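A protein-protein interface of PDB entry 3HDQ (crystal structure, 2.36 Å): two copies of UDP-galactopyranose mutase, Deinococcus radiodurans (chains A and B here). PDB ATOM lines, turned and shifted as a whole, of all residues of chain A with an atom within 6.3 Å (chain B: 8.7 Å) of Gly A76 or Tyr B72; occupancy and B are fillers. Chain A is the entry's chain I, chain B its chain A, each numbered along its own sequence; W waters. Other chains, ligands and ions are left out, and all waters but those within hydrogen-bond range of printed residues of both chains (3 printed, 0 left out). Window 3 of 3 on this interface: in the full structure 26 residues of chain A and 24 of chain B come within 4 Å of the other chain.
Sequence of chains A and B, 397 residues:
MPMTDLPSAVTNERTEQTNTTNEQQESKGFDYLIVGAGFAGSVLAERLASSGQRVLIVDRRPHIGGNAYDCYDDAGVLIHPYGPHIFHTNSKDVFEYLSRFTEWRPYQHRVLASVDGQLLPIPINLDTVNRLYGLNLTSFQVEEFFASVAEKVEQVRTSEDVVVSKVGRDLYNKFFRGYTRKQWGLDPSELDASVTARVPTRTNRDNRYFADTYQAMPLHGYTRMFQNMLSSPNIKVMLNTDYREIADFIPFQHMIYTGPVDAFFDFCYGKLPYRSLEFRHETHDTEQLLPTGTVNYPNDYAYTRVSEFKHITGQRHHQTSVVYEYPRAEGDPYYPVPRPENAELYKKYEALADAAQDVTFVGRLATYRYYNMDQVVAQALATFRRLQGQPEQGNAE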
ATOM      1  N   TYR A  72     -12.400  10.193 -23.798  1.00  0.00           N
ATOM      2  CA  TYR A  72     -13.171   9.812 -24.978  1.00  0.00           C
ATOM      3  C   TYR A  72     -12.876  10.772 -26.114  1.00  0.00           C
ATOM      4  O   TYR A  72     -12.872  11.980 -25.913  1.00  0.00           O
ATOM      5  CB  TYR A  72     -14.676   9.777 -24.667  1.00  0.00           C
ATOM      6  CG  TYR A  72     -15.087   8.577 -23.833  1.00  0.00           C
ATOM      7  CD1 TYR A  72     -15.613   7.430 -24.426  1.00  0.00           C
ATOM      8  CD2 TYR A  72     -14.910   8.575 -22.458  1.00  0.00           C
ATOM      9  CE1 TYR A  72     -15.970   6.333 -23.666  1.00  0.00           C
ATOM     10  CE2 TYR A  72     -15.263   7.479 -21.691  1.00  0.00           C
ATOM     11  CZ  TYR A  72     -15.794   6.363 -22.300  1.00  0.00           C
ATOM     12  OH  TYR A  72     -16.144   5.274 -21.523  1.00  0.00           O
ATOM     13  N   ASP A  73     -12.617  10.235 -27.303  1.00  0.00           N
ATOM     14  CA  ASP A  73     -12.267  11.074 -28.441  1.00  0.00           C
ATOM     15  C   ASP A  73     -13.519  11.604 -29.142  1.00  0.00           C
ATOM     16  O   ASP A  73     -14.633  11.417 -28.652  1.00  0.00           O
ATOM     17  CB  ASP A  73     -11.313  10.357 -29.413  1.00  0.00           C
ATOM     18  CG  ASP A  73     -11.958   9.175 -30.132  1.00  0.00           C
ATOM     19  OD1 ASP A  73     -13.193   8.998 -30.046  1.00  0.00           O
ATOM     20  OD2 ASP A  73     -11.209   8.422 -30.797  1.00  0.00           O
ATOM     21  N   ASP A  74     -13.325  12.284 -30.266  1.00  0.00           N
ATOM     22  CA  ASP A  74     -14.431  12.896 -30.992  1.00  0.00           C
ATOM     23  C   ASP A  74     -15.500  11.889 -31.396  1.00  0.00           C
ATOM     24  O   ASP A  74     -16.683  12.219 -31.423  1.00  0.00           O
ATOM     25  CB  ASP A  74     -13.927  13.672 -32.219  1.00  0.00           C
ATOM     26  CG  ASP A  74     -13.249  14.981 -31.840  1.00  0.00           C
ATOM     27  OD1 ASP A  74     -13.225  15.313 -30.637  1.00  0.00           O
ATOM     28  OD2 ASP A  74     -12.743  15.682 -32.739  1.00  0.00           O
ATOM     29  N   ALA A  75     -15.098  10.661 -31.707  1.00  0.00           N
ATOM     30  CA  ALA A  75     -16.064   9.655 -32.136  1.00  0.00           C
ATOM     31  C   ALA A  75     -16.715   8.895 -30.979  1.00  0.00           C
ATOM     32  O   ALA A  75     -17.650   8.127 -31.188  1.00  0.00           O
ATOM     33  CB  ALA A  75     -15.433   8.694 -33.120  1.00  0.00           C
ATOM     34  N   GLY A  76     -16.235   9.105 -29.761  1.00  0.00           N
ATOM     35  CA  GLY A  76     -16.800   8.416 -28.609  1.00  0.00           C
ATOM     36  C   GLY A  76     -16.048   7.163 -28.192  1.00  0.00           C
ATOM     37  O   GLY A  76     -16.564   6.346 -27.423  1.00  0.00           O
ATOM     38  N   VAL A  77     -14.824   7.011 -28.692  1.00  0.00           N
ATOM     39  CA  VAL A  77     -13.963   5.889 -28.325  1.00  0.00           C
ATOM     40  C   VAL A  77     -13.048   6.294 -27.164  1.00  0.00           C
ATOM     41  O   VAL A  77     -12.481   7.394 -27.167  1.00  0.00           O
ATOM     42  CB  VAL A  77     -13.100   5.464 -29.516  1.00  0.00           C
ATOM     43  CG1 VAL A  77     -12.235   4.256 -29.161  1.00  0.00           C
ATOM     44  CG2 VAL A  77     -13.980   5.179 -30.736  1.00  0.00           C
ATOM     45  N   LEU A  78     -12.919   5.419 -26.168  1.00  0.00           N
ATOM     46  CA  LEU A  78     -11.994   5.656 -25.052  1.00  0.00           C
ATOM     47  C   LEU A  78     -10.560   5.413 -25.514  1.00  0.00           C
ATOM     48  O   LEU A  78     -10.237   4.332 -25.984  1.00  0.00           O
ATOM     49  CB  LEU A  78     -12.336   4.739 -23.865  1.00  0.00           C
ATOM     50  CG  LEU A  78     -11.479   4.785 -22.600  1.00  0.00           C
ATOM     51  CD1 LEU A  78     -11.594   6.139 -21.903  1.00  0.00           C
ATOM     52  CD2 LEU A  78     -11.842   3.644 -21.640  1.00  0.00           C
ATOM     53  N   ARG A 224     -10.992   7.827 -14.444  1.00  0.00           N
ATOM     54  CA  ARG A 224     -11.976   7.517 -13.409  1.00  0.00           C
ATOM     55  C   ARG A 224     -11.316   7.013 -12.124  1.00  0.00           C
ATOM     56  O   ARG A 224     -11.709   7.395 -11.016  1.00  0.00           O
ATOM     57  CB  ARG A 224     -12.991   6.499 -13.937  1.00  0.00           C
ATOM     58  CG  ARG A 224     -13.905   7.069 -15.020  1.00  0.00           C
ATOM     59  CD  ARG A 224     -15.142   7.724 -14.405  1.00  0.00           C
ATOM     60  NE  ARG A 224     -15.821   6.768 -13.528  1.00  0.00           N
ATOM     61  CZ  ARG A 224     -16.813   5.964 -13.911  1.00  0.00           C
ATOM     62  NH1 ARG A 224     -17.280   6.001 -15.160  1.00  0.00           N
ATOM     63  NH2 ARG A 224     -17.346   5.126 -13.035  1.00  0.00           N
ATOM     64  N   GLN A 315     -13.983  -1.847 -24.975  1.00  0.00           N
ATOM     65  CA  GLN A 315     -15.126  -1.047 -25.409  1.00  0.00           C
ATOM     66  C   GLN A 315     -15.757  -1.607 -26.676  1.00  0.00           C
ATOM     67  O   GLN A 315     -15.070  -2.069 -27.586  1.00  0.00           O
ATOM     68  CB  GLN A 315     -14.736   0.403 -25.662  1.00  0.00           C
ATOM     69  CG  GLN A 315     -15.904   1.254 -26.120  1.00  0.00           C
ATOM     70  CD  GLN A 315     -15.497   2.690 -26.381  1.00  0.00           C
ATOM     71  OE1 GLN A 315     -14.323   2.977 -26.624  1.00  0.00           O
ATOM     72  NE2 GLN A 315     -16.463   3.603 -26.324  1.00  0.00           N
ATOM     73  N   HIS A 317     -18.155  -0.660 -29.959  1.00  0.00           N
ATOM     74  CA  HIS A 317     -18.335   0.559 -30.727  1.00  0.00           C
ATOM     75  C   HIS A 317     -18.357   0.179 -32.193  1.00  0.00           C
ATOM     76  O   HIS A 317     -17.719  -0.792 -32.594  1.00  0.00           O
ATOM     77  CB  HIS A 317     -17.153   1.503 -30.470  1.00  0.00           C
ATOM     78  CG  HIS A 317     -17.444   2.942 -30.766  1.00  0.00           C
ATOM     79  ND1 HIS A 317     -17.416   3.460 -32.043  1.00  0.00           N
ATOM     80  CD2 HIS A 317     -17.756   3.974 -29.946  1.00  0.00           C
ATOM     81  CE1 HIS A 317     -17.701   4.751 -31.998  1.00  0.00           C
ATOM     82  NE2 HIS A 317     -17.911   5.089 -30.738  1.00  0.00           N
ATOM     83  N   TYR B  69     -21.994  20.700 -16.810  1.00  0.00           N
ATOM     84  CA  TYR B  69     -20.982  19.679 -17.005  1.00  0.00           C
ATOM     85  C   TYR B  69     -21.607  18.444 -17.645  1.00  0.00           C
ATOM     86  O   TYR B  69     -22.712  18.043 -17.273  1.00  0.00           O
ATOM     87  CB  TYR B  69     -20.391  19.310 -15.647  1.00  0.00           C
ATOM     88  CG  TYR B  69     -19.448  18.128 -15.652  1.00  0.00           C
ATOM     89  CD1 TYR B  69     -18.172  18.241 -16.177  1.00  0.00           C
ATOM     90  CD2 TYR B  69     -19.821  16.918 -15.096  1.00  0.00           C
ATOM     91  CE1 TYR B  69     -17.291  17.173 -16.156  1.00  0.00           C
ATOM     92  CE2 TYR B  69     -18.955  15.844 -15.074  1.00  0.00           C
ATOM     93  CZ  TYR B  69     -17.692  15.981 -15.611  1.00  0.00           C
ATOM     94  OH  TYR B  69     -16.824  14.924 -15.601  1.00  0.00           O
ATOM     95  N   ASP B  70     -20.913  17.843 -18.605  1.00  0.00           N
ATOM     96  CA  ASP B  70     -21.324  16.532 -19.105  1.00  0.00           C
ATOM     97  C   ASP B  70     -20.169  15.521 -19.121  1.00  0.00           C
ATOM     98  O   ASP B  70     -18.997  15.889 -19.056  1.00  0.00           O
ATOM     99  CB  ASP B  70     -22.007  16.631 -20.478  1.00  0.00           C
ATOM    100  CG  ASP B  70     -21.115  17.212 -21.545  1.00  0.00           C
ATOM    101  OD1 ASP B  70     -21.665  17.743 -22.527  1.00  0.00           O
ATOM    102  OD2 ASP B  70     -19.876  17.138 -21.419  1.00  0.00           O
ATOM    103  N   CYS B  71     -20.509  14.246 -19.191  1.00  0.00           N
ATOM    104  CA  CYS B  71     -19.502  13.201 -19.139  1.00  0.00           C
ATOM    105  C   CYS B  71     -20.055  11.886 -19.675  1.00  0.00           C
ATOM    106  O   CYS B  71     -21.270  11.704 -19.816  1.00  0.00           O
ATOM    107  CB  CYS B  71     -19.039  13.003 -17.698  1.00  0.00           C
ATOM    108  SG  CYS B  71     -20.355  12.388 -16.644  1.00  0.00           S
ATOM    109  N   TYR B  72     -19.154  10.969 -19.981  1.00  0.00           N
ATOM    110  CA  TYR B  72     -19.546   9.651 -20.452  1.00  0.00           C
ATOM    111  C   TYR B  72     -19.763   8.729 -19.251  1.00  0.00           C
ATOM    112  O   TYR B  72     -18.927   8.681 -18.342  1.00  0.00           O
ATOM    113  CB  TYR B  72     -18.467   9.097 -21.384  1.00  0.00           C
ATOM    114  CG  TYR B  72     -18.452   9.729 -22.764  1.00  0.00           C
ATOM    115  CD1 TYR B  72     -19.113   9.123 -23.831  1.00  0.00           C
ATOM    116  CD2 TYR B  72     -17.777  10.920 -23.004  1.00  0.00           C
ATOM    117  CE1 TYR B  72     -19.101   9.685 -25.095  1.00  0.00           C
ATOM    118  CE2 TYR B  72     -17.765  11.491 -24.276  1.00  0.00           C
ATOM    119  CZ  TYR B  72     -18.429  10.865 -25.313  1.00  0.00           C
ATOM    120  OH  TYR B  72     -18.431  11.407 -26.581  1.00  0.00           O
ATOM    121  N   ASP B  73     -20.884   8.007 -19.239  1.00  0.00           N
ATOM    122  CA  ASP B  73     -21.214   7.138 -18.104  1.00  0.00           C
ATOM    123  C   ASP B  73     -20.563   5.754 -18.208  1.00  0.00           C
ATOM    124  O   ASP B  73     -19.780   5.505 -19.118  1.00  0.00           O
ATOM    125  CB  ASP B  73     -22.733   7.012 -17.924  1.00  0.00           C
ATOM    126  CG  ASP B  73     -23.422   6.304 -19.088  1.00  0.00           C
ATOM    127  OD1 ASP B  73     -22.775   5.612 -19.912  1.00  0.00           O
ATOM    128  OD2 ASP B  73     -24.652   6.441 -19.164  1.00  0.00           O
ATOM    129  N   ASP B  74     -20.891   4.861 -17.280  1.00  0.00           N
ATOM    130  CA  ASP B  74     -20.266   3.534 -17.250  1.00  0.00           C
ATOM    131  C   ASP B  74     -20.445   2.776 -18.567  1.00  0.00           C
ATOM    132  O   ASP B  74     -19.587   1.972 -18.954  1.00  0.00           O
ATOM    133  CB  ASP B  74     -20.810   2.698 -16.091  1.00  0.00           C
ATOM    134  CG  ASP B  74     -20.263   3.147 -14.742  1.00  0.00           C
ATOM    135  OD1 ASP B  74     -19.433   4.085 -14.709  1.00  0.00           O
ATOM    136  OD2 ASP B  74     -20.657   2.559 -13.715  1.00  0.00           O
ATOM    137  N   ALA B  75     -21.552   3.043 -19.258  1.00  0.00           N
ATOM    138  CA  ALA B  75     -21.869   2.330 -20.498  1.00  0.00           C
ATOM    139  C   ALA B  75     -21.286   3.005 -21.736  1.00  0.00           C
ATOM    140  O   ALA B  75     -21.416   2.485 -22.844  1.00  0.00           O
ATOM    141  CB  ALA B  75     -23.375   2.172 -20.647  1.00  0.00           C
ATOM    142  N   GLY B  76     -20.668   4.168 -21.553  1.00  0.00           N
ATOM    143  CA  GLY B  76     -20.131   4.923 -22.671  1.00  0.00           C
ATOM    144  C   GLY B  76     -21.138   5.851 -23.342  1.00  0.00           C
ATOM    145  O   GLY B  76     -20.964   6.226 -24.500  1.00  0.00           O
ATOM    146  N   VAL B  77     -22.201   6.214 -22.626  1.00  0.00           N
ATOM    147  CA  VAL B  77     -23.171   7.171 -23.155  1.00  0.00           C
ATOM    148  C   VAL B  77     -22.891   8.578 -22.608  1.00  0.00           C
ATOM    149  O   VAL B  77     -22.721   8.758 -21.411  1.00  0.00           O
ATOM    150  CB  VAL B  77     -24.629   6.758 -22.825  1.00  0.00           C
ATOM    151  CG1 VAL B  77     -25.622   7.788 -23.380  1.00  0.00           C
ATOM    152  CG2 VAL B  77     -24.932   5.373 -23.382  1.00  0.00           C
ATOM    153  N   LEU B  78     -22.824   9.562 -23.495  1.00  0.00           N
ATOM    154  CA  LEU B  78     -22.661  10.956 -23.095  1.00  0.00           C
ATOM    155  C   LEU B  78     -23.910  11.459 -22.372  1.00  0.00           C
ATOM    156  O   LEU B  78     -24.985  11.472 -22.952  1.00  0.00           O
ATOM    157  CB  LEU B  78     -22.392  11.817 -24.329  1.00  0.00           C
ATOM    158  CG  LEU B  78     -22.107  13.307 -24.117  1.00  0.00           C
ATOM    159  CD1 LEU B  78     -20.852  13.520 -23.255  1.00  0.00           C
ATOM    160  CD2 LEU B  78     -21.964  13.997 -25.460  1.00  0.00           C
ATOM    161  N   ILE B  79     -23.772  11.855 -21.105  1.00  0.00           N
ATOM    162  CA  ILE B  79     -24.914  12.304 -20.298  1.00  0.00           C
ATOM    163  C   ILE B  79     -24.673  13.648 -19.621  1.00  0.00           C
ATOM    164  O   ILE B  79     -23.547  14.163 -19.594  1.00  0.00           O
ATOM    165  CB  ILE B  79     -25.215  11.330 -19.158  1.00  0.00           C
ATOM    166  CG1 ILE B  79     -24.033  11.335 -18.175  1.00  0.00           C
ATOM    167  CG2 ILE B  79     -25.524   9.949 -19.706  1.00  0.00           C
ATOM    168  CD1 ILE B  79     -24.275  10.638 -16.881  1.00  0.00           C
ATOM    169  N   HIS B  80     -25.740  14.208 -19.064  1.00  0.00           N
ATOM    170  CA  HIS B  80     -25.632  15.398 -18.213  1.00  0.00           C
ATOM    171  C   HIS B  80     -25.965  15.014 -16.777  1.00  0.00           C
ATOM    172  O   HIS B  80     -27.132  14.797 -16.440  1.00  0.00           O
ATOM    173  CB  HIS B  80     -26.582  16.501 -18.683  1.00  0.00           C
ATOM    174  CG  HIS B  80     -26.481  16.808 -20.145  1.00  0.00           C
ATOM    175  ND1 HIS B  80     -27.333  17.684 -20.782  1.00  0.00           N
ATOM    176  CD2 HIS B  80     -25.635  16.344 -21.098  1.00  0.00           C
ATOM    177  CE1 HIS B  80     -27.013  17.755 -22.063  1.00  0.00           C
ATOM    178  NE2 HIS B  80     -25.985  16.951 -22.281  1.00  0.00           N
ATOM    179  N   PRO B  81     -24.944  14.919 -15.923  1.00  0.00           N
ATOM    180  CA  PRO B  81     -25.199  14.484 -14.542  1.00  0.00           C
ATOM    181  C   PRO B  81     -26.248  15.331 -13.811  1.00  0.00           C
ATOM    182  O   PRO B  81     -26.913  14.787 -12.930  1.00  0.00           O
ATOM    183  CB  PRO B  81     -23.829  14.616 -13.859  1.00  0.00           C
ATOM    184  CG  PRO B  81     -22.834  14.530 -14.996  1.00  0.00           C
ATOM    185  CD  PRO B  81     -23.519  15.180 -16.182  1.00  0.00           C
ATOM    186  N   LEU B 219     -21.025  20.235 -30.234  1.00  0.00           N
ATOM    187  CA  LEU B 219     -20.822  18.997 -30.987  1.00  0.00           C
ATOM    188  C   LEU B 219     -20.220  17.853 -30.153  1.00  0.00           C
ATOM    189  O   LEU B 219     -20.660  16.704 -30.258  1.00  0.00           O
ATOM    190  CB  LEU B 219     -20.005  19.247 -32.255  1.00  0.00           C
ATOM    191  CG  LEU B 219     -19.811  18.030 -33.175  1.00  0.00           C
ATOM    192  CD1 LEU B 219     -21.146  17.534 -33.697  1.00  0.00           C
ATOM    193  CD2 LEU B 219     -18.900  18.368 -34.343  1.00  0.00           C
ATOM    194  N   HIS B 220     -19.241  18.158 -29.309  1.00  0.00           N
ATOM    195  CA  HIS B 220     -18.670  17.116 -28.458  1.00  0.00           C
ATOM    196  C   HIS B 220     -18.986  17.300 -26.984  1.00  0.00           C
ATOM    197  O   HIS B 220     -18.277  16.790 -26.110  1.00  0.00           O
ATOM    198  CB  HIS B 220     -17.170  17.011 -28.696  1.00  0.00           C
ATOM    199  CG  HIS B 220     -16.811  16.892 -30.145  1.00  0.00           C
ATOM    200  ND1 HIS B 220     -17.194  15.820 -30.922  1.00  0.00           N
ATOM    201  CD2 HIS B 220     -16.114  17.718 -30.962  1.00  0.00           C
ATOM    202  CE1 HIS B 220     -16.751  15.991 -32.155  1.00  0.00           C
ATOM    203  NE2 HIS B 220     -16.085  17.130 -32.199  1.00  0.00           N
ATOM    204  N   GLY B 221     -20.063  18.035 -26.714  1.00  0.00           N
ATOM    205  CA  GLY B 221     -20.532  18.240 -25.361  1.00  0.00           C
ATOM    206  C   GLY B 221     -20.002  19.505 -24.711  1.00  0.00           C
ATOM    207  O   GLY B 221     -19.065  20.133 -25.202  1.00  0.00           O
ATOM    208  N   THR B 223     -18.459  19.900 -21.724  1.00  0.00           N
ATOM    209  CA  THR B 223     -17.188  19.813 -21.021  1.00  0.00           C
ATOM    210  C   THR B 223     -16.009  20.135 -21.935  1.00  0.00           C
ATOM    211  O   THR B 223     -15.132  20.937 -21.574  1.00  0.00           O
ATOM    212  CB  THR B 223     -17.030  18.454 -20.317  1.00  0.00           C
ATOM    213  OG1 THR B 223     -18.019  18.365 -19.291  1.00  0.00           O
ATOM    214  CG2 THR B 223     -15.642  18.304 -19.695  1.00  0.00           C
ATOM    215  N   ARG B 224     -16.005  19.531 -23.118  1.00  0.00           N
ATOM    216  CA  ARG B 224     -15.035  19.874 -24.149  1.00  0.00           C
ATOM    217  C   ARG B 224     -15.009  21.384 -24.429  1.00  0.00           C
ATOM    218  O   ARG B 224     -13.941  21.977 -24.537  1.00  0.00           O
ATOM    219  CB  ARG B 224     -15.322  19.084 -25.430  1.00  0.00           C
ATOM    220  CG  ARG B 224     -15.042  17.593 -25.271  1.00  0.00           C
ATOM    221  CD  ARG B 224     -13.558  17.313 -25.388  1.00  0.00           C
ATOM    222  NE  ARG B 224     -13.088  17.761 -26.698  1.00  0.00           N
ATOM    223  CZ  ARG B 224     -13.210  17.045 -27.815  1.00  0.00           C
ATOM    224  NH1 ARG B 224     -13.771  15.838 -27.781  1.00  0.00           N
ATOM    225  NH2 ARG B 224     -12.766  17.536 -28.967  1.00  0.00           N
ATOM    226  N   THR B 313     -27.935  14.702 -27.676  1.00  0.00           N
ATOM    227  CA  THR B 313     -26.550  14.697 -28.142  1.00  0.00           C
ATOM    228  C   THR B 313     -26.405  14.213 -29.583  1.00  0.00           C
ATOM    229  O   THR B 313     -25.414  14.500 -30.241  1.00  0.00           O
ATOM    230  CB  THR B 313     -25.673  13.779 -27.268  1.00  0.00           C
ATOM    231  OG1 THR B 313     -26.109  12.423 -27.425  1.00  0.00           O
ATOM    232  CG2 THR B 313     -25.782  14.179 -25.798  1.00  0.00           C
ATOM    233  N   GLN B 315     -25.752  11.267 -30.161  1.00  0.00           N
ATOM    234  CA  GLN B 315     -24.841  10.124 -30.073  1.00  0.00           C
ATOM    235  C   GLN B 315     -25.462   8.835 -30.613  1.00  0.00           C
ATOM    236  O   GLN B 315     -26.636   8.558 -30.381  1.00  0.00           O
ATOM    237  CB  GLN B 315     -24.384   9.883 -28.627  1.00  0.00           C
ATOM    238  CG  GLN B 315     -23.326   8.792 -28.486  1.00  0.00           C
ATOM    239  CD  GLN B 315     -22.989   8.461 -27.042  1.00  0.00           C
ATOM    240  OE1 GLN B 315     -23.685   8.878 -26.108  1.00  0.00           O
ATOM    241  NE2 GLN B 315     -21.910   7.701 -26.851  1.00  0.00           N
ATOM    242  N   ARG B 316     -24.655   8.042 -31.315  1.00  0.00           N
ATOM    243  CA  ARG B 316     -25.045   6.689 -31.719  1.00  0.00           C
ATOM    244  C   ARG B 316     -24.510   5.654 -30.720  1.00  0.00           C
ATOM    245  O   ARG B 316     -23.352   5.716 -30.336  1.00  0.00           O
ATOM    246  CB  ARG B 316     -24.498   6.388 -33.116  1.00  0.00           C
ATOM    247  CG  ARG B 316     -24.936   5.043 -33.658  1.00  0.00           C
ATOM    248  CD  ARG B 316     -24.234   4.685 -34.960  1.00  0.00           C
ATOM    249  NE  ARG B 316     -24.363   3.256 -35.233  1.00  0.00           N
ATOM    250  CZ  ARG B 316     -24.126   2.687 -36.411  1.00  0.00           C
ATOM    251  NH1 ARG B 316     -23.748   3.426 -37.448  1.00  0.00           N
ATOM    252  NH2 ARG B 316     -24.271   1.376 -36.551  1.00  0.00           N
ATOM    253  N   HIS B 317     -25.340   4.697 -30.317  1.00  0.00           N
ATOM    254  CA  HIS B 317     -24.953   3.735 -29.293  1.00  0.00           C
ATOM    255  C   HIS B 317     -26.023   2.643 -29.259  1.00  0.00           C
ATOM    256  O   HIS B 317     -27.173   2.906 -29.588  1.00  0.00           O
ATOM    257  CB  HIS B 317     -24.883   4.441 -27.936  1.00  0.00           C
ATOM    258  CG  HIS B 317     -24.113   3.698 -26.884  1.00  0.00           C
ATOM    259  ND1 HIS B 317     -24.597   2.566 -26.260  1.00  0.00           N
ATOM    260  CD2 HIS B 317     -22.912   3.959 -26.307  1.00  0.00           C
ATOM    261  CE1 HIS B 317     -23.720   2.150 -25.362  1.00  0.00           C
ATOM    262  NE2 HIS B 317     -22.691   2.982 -25.366  1.00  0.00           N
ATOM    263  N   SER B 321     -29.121   5.922 -22.218  1.00  0.00           N
ATOM    264  CA  SER B 321     -29.152   6.382 -20.833  1.00  0.00           C
ATOM    265  C   SER B 321     -30.162   7.509 -20.629  1.00  0.00           C
ATOM    266  O   SER B 321     -30.255   8.441 -21.435  1.00  0.00           O
ATOM    267  CB  SER B 321     -27.766   6.848 -20.372  1.00  0.00           C
ATOM    268  OG  SER B 321     -26.868   5.771 -20.309  1.00  0.00           O
HETATM  269  O   HOH W   1     -14.821  13.991 -26.020  1.00  0.00           O
HETATM  270  O   HOH W   2     -20.121   6.686 -28.995  1.00  0.00           O
HETATM  271  O   HOH W   3     -18.713  13.696 -29.436  1.00  0.00           O
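NH2 of Arg A224 lies within salt-bridge range of OD1 of Asp B74 (2.9 Å). The guanidinium group (NH2) of Arg B224 lies within salt-bridge range of the side-chain carboxylate (OD1) of Asp A74, 2.8 Å away.
The side-chain carboxylate (OD1) of Asp A73 is in hydrogen-bond range of the backbone NH (N) of Gly A76, 3.1 Å away. The backbone carbonyl oxygen (O) of Gly A76 is in hydrogen-bond range of the side-chain amide nitrogen (NE2) of Gln A315.
Water W1 lies within hydrogen-bond range of NH1 of Arg B224 (2.8 Å) and O of Tyr A72 (2.8 Å). Water W2 lies within hydrogen-bond range of the side-chain amide nitrogen of Gln B315 and a ring nitrogen (NE2) of His A317. Water W3 lies within hydrogen-bond range of a ring nitrogen (ND1) of His B220 (3.0 Å) and the backbone carbonyl oxygen of Asp A74 (3.2 Å).
Tyr A72 touches its own counterpart, Tyr B72. Asp A74 touches Arg B224, and with the chains exchanged Arg A224 touches Asp B74. Gly A76 touches Tyr B72, but with the chains exchanged Tyr A72 does not touch Gly B76 (4.2 Å). Of the 5 pairs that touch across the chains among the printed residues, 3 have their exchanged pair printed and touching as well.
Of the printed residues of chain B, Tyr A72 touches Tyr B72. Of the printed residues of chain B, Asp A74 touches His B220 and Arg B224. No residue of chain B comes within 4 Å of Ala A75. Of chain B, only Tyr B72 (3.96 Å) comes within 4 Å of Gly A76. Tyr B72 touches just these residues of chain A: Tyr A72 (3.6 Å) and Gly A76 (3.96 Å). Of the printed residues of chain A, Asp B74 touches Arg A224. Printed residues of chain A within 4 Å of His B220: Asp A74 (3.6 Å). Of the printed residues of chain A, Arg B224 touches Asp A74. The nearest residue of chain A that does not touch Tyr B72 is Asp A73 (4.3 Å).
Printed residues of chain B that touch a printed residue of chain A: Tyr B72, Asp B74, His B220 and Arg B224. Among the printed residues, 5 pairs touch across the chains.
Tyr B72 touches Tyr A72 (CE2 to CB, 3.6 Å). His B220 touches Asp A74. Tyr B72 touches Gly A76 (OH to CA, 3.96 Å).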
